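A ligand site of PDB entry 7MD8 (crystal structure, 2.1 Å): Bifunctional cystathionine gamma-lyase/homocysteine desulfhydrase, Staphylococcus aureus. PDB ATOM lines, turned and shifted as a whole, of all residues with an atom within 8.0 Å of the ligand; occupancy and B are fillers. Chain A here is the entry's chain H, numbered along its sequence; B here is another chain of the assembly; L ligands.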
ATOM      1  N   SER A   1       5.340 -15.734  16.878  1.00  0.00           N
ATOM      2  CA  SER A   1       4.273 -16.674  17.179  1.00  0.00           C
ATOM      3  C   SER A   1       3.053 -15.902  17.683  1.00  0.00           C
ATOM      4  O   SER A   1       2.306 -15.353  16.884  1.00  0.00           O
ATOM      5  CB  SER A   1       4.750 -17.703  18.204  1.00  0.00           C
ATOM      6  OG  SER A   1       3.704 -18.566  18.615  1.00  0.00           O
ATOM      7  N   ASN A   2       2.837 -15.849  19.000  1.00  0.00           N
ATOM      8  CA  ASN A   2       1.693 -15.112  19.502  1.00  0.00           C
ATOM      9  C   ASN A   2       1.941 -13.609  19.434  1.00  0.00           C
ATOM     10  O   ASN A   2       3.057 -13.142  19.185  1.00  0.00           O
ATOM     11  CB  ASN A   2       1.347 -15.566  20.917  1.00  0.00           C
ATOM     12  CG  ASN A   2       0.762 -16.962  20.947  1.00  0.00           C
ATOM     13  OD1 ASN A   2       0.113 -17.390  19.992  1.00  0.00           O
ATOM     14  ND2 ASN A   2       0.991 -17.680  22.036  1.00  0.00           N
ATOM     15  N   LYS A   3       0.863 -12.835  19.647  1.00  0.00           N
ATOM     16  CA  LYS A   3       0.870 -11.401  19.333  1.00  0.00           C
ATOM     17  C   LYS A   3       1.887 -10.633  20.183  1.00  0.00           C
ATOM     18  O   LYS A   3       2.615  -9.769  19.674  1.00  0.00           O
ATOM     19  CB  LYS A   3      -0.521 -10.816  19.531  1.00  0.00           C
ATOM     20  CG  LYS A   3      -1.613 -11.526  18.749  1.00  0.00           C
ATOM     21  CD  LYS A   3      -2.895 -10.672  18.623  1.00  0.00           C
ATOM     22  CE  LYS A   3      -3.688 -10.611  19.933  1.00  0.00           C
ATOM     23  NZ  LYS A   3      -5.076 -10.062  19.712  1.00  0.00           N
ATOM     24  N   LYS A   4       1.940 -10.918  21.479  1.00  0.00           N
ATOM     25  CA  LYS A   4       2.853 -10.175  22.342  1.00  0.00           C
ATOM     26  C   LYS A   4       4.303 -10.443  21.983  1.00  0.00           C
ATOM     27  O   LYS A   4       5.164  -9.587  22.213  1.00  0.00           O
ATOM     28  CB  LYS A   4       2.594 -10.538  23.806  1.00  0.00           C
ATOM     29  CG  LYS A   4       1.309  -9.950  24.369  1.00  0.00           C
ATOM     30  CD  LYS A   4       1.165 -10.420  25.815  1.00  0.00           C
ATOM     31  CE  LYS A   4      -0.167 -10.062  26.391  1.00  0.00           C
ATOM     32  NZ  LYS A   4      -0.369 -10.726  27.710  1.00  0.00           N
ATOM     33  N   THR A   5       4.598 -11.611  21.423  1.00  0.00           N
ATOM     34  CA  THR A   5       5.948 -11.915  20.983  1.00  0.00           C
ATOM     35  C   THR A   5       6.253 -11.179  19.684  1.00  0.00           C
ATOM     36  O   THR A   5       7.319 -10.558  19.538  1.00  0.00           O
ATOM     37  CB  THR A   5       6.114 -13.428  20.803  1.00  0.00           C
ATOM     38  OG1 THR A   5       5.741 -14.079  22.015  1.00  0.00           O
ATOM     39  CG2 THR A   5       7.548 -13.797  20.452  1.00  0.00           C
ATOM     40  N   LYS A   6       5.319 -11.226  18.731  1.00  0.00           N
ATOM     41  CA  LYS A   6       5.446 -10.494  17.481  1.00  0.00           C
ATOM     42  C   LYS A   6       5.718  -9.017  17.735  1.00  0.00           C
ATOM     43  O   LYS A   6       6.541  -8.402  17.048  1.00  0.00           O
ATOM     44  CB  LYS A   6       4.180 -10.683  16.650  1.00  0.00           C
ATOM     45  CG  LYS A   6       4.299 -10.371  15.185  1.00  0.00           C
ATOM     46  CD  LYS A   6       3.004 -10.771  14.459  1.00  0.00           C
ATOM     47  CE  LYS A   6       2.962 -10.289  13.019  1.00  0.00           C
ATOM     48  NZ  LYS A   6       1.633 -10.579  12.414  1.00  0.00           N
ATOM     49  N   LEU A   7       5.045  -8.436  18.739  1.00  0.00           N
ATOM     50  CA  LEU A   7       5.289  -7.027  19.069  1.00  0.00           C
ATOM     51  C   LEU A   7       6.744  -6.760  19.444  1.00  0.00           C
ATOM     52  O   LEU A   7       7.254  -5.666  19.181  1.00  0.00           O
ATOM     53  CB  LEU A   7       4.378  -6.608  20.221  1.00  0.00           C
ATOM     54  CG  LEU A   7       2.932  -6.348  19.821  1.00  0.00           C
ATOM     55  CD1 LEU A   7       2.090  -6.204  21.054  1.00  0.00           C
ATOM     56  CD2 LEU A   7       2.869  -5.109  18.941  1.00  0.00           C
ATOM     57  N   ILE A   8       7.401  -7.718  20.069  1.00  0.00           N
ATOM     58  CA  ILE A   8       8.772  -7.485  20.530  1.00  0.00           C
ATOM     59  C   ILE A   8       9.776  -7.806  19.436  1.00  0.00           C
ATOM     60  O   ILE A   8      10.721  -7.047  19.202  1.00  0.00           O
ATOM     61  CB  ILE A   8       9.041  -8.326  21.798  1.00  0.00           C
ATOM     62  CG1 ILE A   8       8.035  -7.945  22.891  1.00  0.00           C
ATOM     63  CG2 ILE A   8      10.492  -8.132  22.280  1.00  0.00           C
ATOM     64  CD1 ILE A   8       7.999  -6.441  23.173  1.00  0.00           C
ATOM     65  N   HIS A   9       9.568  -8.894  18.721  1.00  0.00           N
ATOM     66  CA  HIS A   9      10.577  -9.364  17.791  1.00  0.00           C
ATOM     67  C   HIS A   9      10.221  -9.120  16.316  1.00  0.00           C
ATOM     68  O   HIS A   9      11.066  -9.375  15.459  1.00  0.00           O
ATOM     69  CB  HIS A   9      10.849 -10.852  18.056  1.00  0.00           C
ATOM     70  CG  HIS A   9      11.397 -11.096  19.419  1.00  0.00           C
ATOM     71  ND1 HIS A   9      12.715 -10.836  19.747  1.00  0.00           N
ATOM     72  CD2 HIS A   9      10.801 -11.504  20.563  1.00  0.00           C
ATOM     73  CE1 HIS A   9      12.907 -11.098  21.027  1.00  0.00           C
ATOM     74  NE2 HIS A   9      11.770 -11.513  21.544  1.00  0.00           N
ATOM     75  N   GLY A  10       9.017  -8.605  16.023  1.00  0.00           N
ATOM     76  CA  GLY A  10       8.644  -8.350  14.640  1.00  0.00           C
ATOM     77  C   GLY A  10       9.231  -7.051  14.107  1.00  0.00           C
ATOM     78  O   GLY A  10       9.355  -6.057  14.809  1.00  0.00           O
ATOM     79  N   GLY A  11       9.583  -7.065  12.818  1.00  0.00           N
ATOM     80  CA  GLY A  11      10.262  -5.928  12.237  1.00  0.00           C
ATOM     81  C   GLY A  11      11.753  -5.940  12.553  1.00  0.00           C
ATOM     82  O   GLY A  11      12.254  -6.780  13.305  1.00  0.00           O
ATOM     83  N   THR A  62       5.024  -5.416   9.406  1.00  0.00           N
ATOM     84  CA  THR A  62       4.945  -6.721  10.053  1.00  0.00           C
ATOM     85  C   THR A  62       3.659  -6.875  10.856  1.00  0.00           C
ATOM     86  O   THR A  62       2.986  -7.911  10.782  1.00  0.00           O
ATOM     87  CB  THR A  62       6.170  -6.932  10.967  1.00  0.00           C
ATOM     88  OG1 THR A  62       7.370  -6.998  10.196  1.00  0.00           O
ATOM     89  CG2 THR A  62       6.019  -8.206  11.752  1.00  0.00           C
ATOM     90  N   LEU A  63       3.326  -5.883  11.673  1.00  0.00           N
ATOM     91  CA  LEU A  63       2.176  -5.985  12.570  1.00  0.00           C
ATOM     92  C   LEU A  63       0.852  -6.078  11.814  1.00  0.00           C
ATOM     93  O   LEU A  63      -0.113  -6.702  12.303  1.00  0.00           O
ATOM     94  CB  LEU A  63       2.164  -4.798  13.526  1.00  0.00           C
ATOM     95  CG  LEU A  63       3.287  -4.662  14.562  1.00  0.00           C
ATOM     96  CD1 LEU A  63       3.004  -3.461  15.463  1.00  0.00           C
ATOM     97  CD2 LEU A  63       3.445  -5.932  15.400  1.00  0.00           C
ATOM     98  N   GLU A  64       0.754  -5.469  10.630  1.00  0.00           N
ATOM     99  CA  GLU A  64      -0.466  -5.564   9.829  1.00  0.00           C
ATOM    100  C   GLU A  64      -0.407  -6.673   8.773  1.00  0.00           C
ATOM    101  O   GLU A  64      -1.297  -6.744   7.923  1.00  0.00           O
ATOM    102  CB  GLU A  64      -0.759  -4.212   9.161  1.00  0.00           C
ATOM    103  CG  GLU A  64      -1.196  -3.086  10.107  1.00  0.00           C
ATOM    104  CD  GLU A  64      -2.633  -3.254  10.668  1.00  0.00           C
ATOM    105  OE1 GLU A  64      -3.214  -4.369  10.612  1.00  0.00           O
ATOM    106  OE2 GLU A  64      -3.168  -2.259  11.208  1.00  0.00           O
ATOM    107  N   ASN A  65       0.621  -7.522   8.818  1.00  0.00           N
ATOM    108  CA  ASN A  65       0.813  -8.585   7.819  1.00  0.00           C
ATOM    109  C   ASN A  65       0.832  -8.039   6.393  1.00  0.00           C
ATOM    110  O   ASN A  65       0.295  -8.628   5.464  1.00  0.00           O
ATOM    111  CB  ASN A  65      -0.242  -9.691   7.969  1.00  0.00           C
ATOM    112  CG  ASN A  65      -0.177 -10.348   9.336  1.00  0.00           C
ATOM    113  OD1 ASN A  65       0.904 -10.655   9.836  1.00  0.00           O
ATOM    114  ND2 ASN A  65      -1.352 -10.549   9.956  1.00  0.00           N
ATOM    115  N   ASN A 181      -6.835  -6.643  11.753  1.00  0.00           N
ATOM    116  CA  ASN A 181      -5.867  -6.608  10.654  1.00  0.00           C
ATOM    117  C   ASN A 181      -6.600  -6.576   9.326  1.00  0.00           C
ATOM    118  O   ASN A 181      -6.883  -7.632   8.726  1.00  0.00           O
ATOM    119  CB  ASN A 181      -4.923  -7.800  10.761  1.00  0.00           C
ATOM    120  CG  ASN A 181      -4.224  -7.862  12.111  1.00  0.00           C
ATOM    121  OD1 ASN A 181      -4.433  -8.790  12.894  1.00  0.00           O
ATOM    122  ND2 ASN A 181      -3.428  -6.838  12.407  1.00  0.00           N
ATOM    123  N   ASP A 184      -5.565  -8.639   6.149  1.00  0.00           N
ATOM    124  CA  ASP A 184      -5.906 -10.049   6.165  1.00  0.00           C
ATOM    125  C   ASP A 184      -7.317 -10.305   5.667  1.00  0.00           C
ATOM    126  O   ASP A 184      -7.648 -11.448   5.346  1.00  0.00           O
ATOM    127  CB  ASP A 184      -5.806 -10.633   7.580  1.00  0.00           C
ATOM    128  CG  ASP A 184      -4.379 -10.896   8.020  1.00  0.00           C
ATOM    129  OD1 ASP A 184      -3.467 -10.862   7.158  1.00  0.00           O
ATOM    130  OD2 ASP A 184      -4.183 -11.140   9.224  1.00  0.00           O
ATOM    131  N   SER B 316      14.676 -19.284  20.237  1.00  0.00           N
ATOM    132  CA  SER B 316      14.322 -18.277  19.255  1.00  0.00           C
ATOM    133  C   SER B 316      14.107 -16.899  19.874  1.00  0.00           C
ATOM    134  O   SER B 316      14.405 -15.892  19.239  1.00  0.00           O
ATOM    135  CB  SER B 316      13.062 -18.718  18.507  1.00  0.00           C
ATOM    136  OG  SER B 316      13.407 -19.659  17.497  1.00  0.00           O
ATOM    137  N   TYR B 317      13.634 -16.852  21.123  1.00  0.00           N
ATOM    138  CA  TYR B 317      13.139 -15.624  21.721  1.00  0.00           C
ATOM    139  C   TYR B 317      13.966 -15.132  22.906  1.00  0.00           C
ATOM    140  O   TYR B 317      13.584 -14.146  23.529  1.00  0.00           O
ATOM    141  CB  TYR B 317      11.677 -15.828  22.167  1.00  0.00           C
ATOM    142  CG  TYR B 317      10.786 -16.269  21.015  1.00  0.00           C
ATOM    143  CD1 TYR B 317      10.797 -15.585  19.810  1.00  0.00           C
ATOM    144  CD2 TYR B 317       9.936 -17.365  21.134  1.00  0.00           C
ATOM    145  CE1 TYR B 317      10.000 -15.971  18.747  1.00  0.00           C
ATOM    146  CE2 TYR B 317       9.117 -17.769  20.059  1.00  0.00           C
ATOM    147  CZ  TYR B 317       9.164 -17.059  18.869  1.00  0.00           C
ATOM    148  OH  TYR B 317       8.378 -17.414  17.789  1.00  0.00           O
ATOM    149  N   GLU B 364       7.467 -10.873  26.157  1.00  0.00           N
ATOM    150  CA  GLU B 364       6.905 -11.700  25.108  1.00  0.00           C
ATOM    151  C   GLU B 364       5.778 -12.572  25.659  1.00  0.00           C
ATOM    152  O   GLU B 364       5.563 -12.660  26.876  1.00  0.00           O
ATOM    153  CB  GLU B 364       7.980 -12.590  24.481  1.00  0.00           C
ATOM    154  CG  GLU B 364       9.089 -11.817  23.839  1.00  0.00           C
ATOM    155  CD  GLU B 364      10.305 -11.712  24.734  1.00  0.00           C
ATOM    156  OE1 GLU B 364      10.158 -11.835  25.956  1.00  0.00           O
ATOM    157  OE2 GLU B 364      11.414 -11.505  24.193  1.00  0.00           O
ATOM    158  N   ASP B 368       4.828 -18.614  24.411  1.00  0.00           N
ATOM    159  CA  ASP B 368       6.009 -18.618  23.550  1.00  0.00           C
ATOM    160  C   ASP B 368       7.295 -18.741  24.366  1.00  0.00           C
ATOM    161  O   ASP B 368       8.200 -19.497  23.996  1.00  0.00           O
ATOM    162  CB  ASP B 368       6.037 -17.368  22.690  1.00  0.00           C
ATOM    163  CG  ASP B 368       4.949 -17.381  21.620  1.00  0.00           C
ATOM    164  OD1 ASP B 368       4.480 -18.468  21.237  1.00  0.00           O
ATOM    165  OD2 ASP B 368       4.576 -16.288  21.153  1.00  0.00           O
HETATM  166  N1  LIG L   1       7.131 -12.476  13.269  1.00  0.00           N
HETATM  167  C1  LIG L   1       7.492 -12.698  14.539  1.00  0.00           C
HETATM  168  C2  LIG L   1       8.689 -11.981  15.099  1.00  0.00           C
HETATM  169  C3  LIG L   1       6.757 -13.583  15.332  1.00  0.00           C
HETATM  170  O1  LIG L   1       7.139 -13.787  16.613  1.00  0.00           O
HETATM  171  C4  LIG L   1       5.644 -14.250  14.816  1.00  0.00           C
HETATM  172  C5  LIG L   1       4.872 -15.196  15.641  1.00  0.00           C
HETATM  173  C6  LIG L   1       5.287 -14.010  13.470  1.00  0.00           C
HETATM  174  C7  LIG L   1       6.064 -13.116  12.748  1.00  0.00           C
HETATM  175  C8  LIG L   1       4.112 -14.687  12.810  1.00  0.00           C
HETATM  176  O2  LIG L   1       3.073 -13.776  12.476  1.00  0.00           O
HETATM  177  P1  LIG L   1       1.570 -14.285  12.228  1.00  0.00           P
HETATM  178  O3  LIG L   1       1.146 -14.011  10.798  1.00  0.00           O
HETATM  179  O4  LIG L   1       1.528 -15.773  12.497  1.00  0.00           O
HETATM  180  O5  LIG L   1       0.641 -13.581  13.184  1.00  0.00           O
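The backbone NH of Ser 1 is covalently linked to a carbon (C5) of the ligand, at 1.4 Å. NZ of Lys 6 is in salt-bridge range of O5 of the ligand. OD1 of Asn 65 lies close to O3 of the ligand, 3.5 Å away.
The side-chain hydroxyl (OG) of Ser 1 lies within hydrogen-bond range of the side-chain carboxylate (OD1) of Asp 368 of chain B. The side-chain amino group of Lys 6 is in hydrogen-bond range of the side-chain amide oxygen of Asn 65 (2.7 Å). The side-chain amino group of Lys 6 sits close to the backbone carbonyl oxygen of Thr 62 (3.4 Å). The side-chain carboxylate (OE2) of Glu 364 of chain B sits at hydrogen-bond distance from a ring nitrogen (NE2) of His 9 (2.7 Å). The side-chain carboxylate (OD2) of Asp 184 sits at hydrogen-bond distance from the side-chain amide nitrogen (ND2) of Asn 65 (3.0 Å). OG1 of Thr 5 is in hydrogen-bond range of OD2 of Asp 368 of chain B. N of Asn 2 is in hydrogen-bond range of OD2 of Asp 368 of chain B (2.8 Å).
Asn 2 touches the ligand. Thr 5 touches the ligand (CG2 to O1, 3.9 Å). His 9 touches the ligand (C to C2, 3.5 Å). N of Gly 10 touches C2 of the ligand, 3.5 Å away. Hydrophobic or aromatic side chains within 4 Å of the ligand: His 9. Within 4 Å of the ligand: Ser 1, Asn 2, Thr 5, Lys 6, His 9, Gly 10 and Asn 65.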
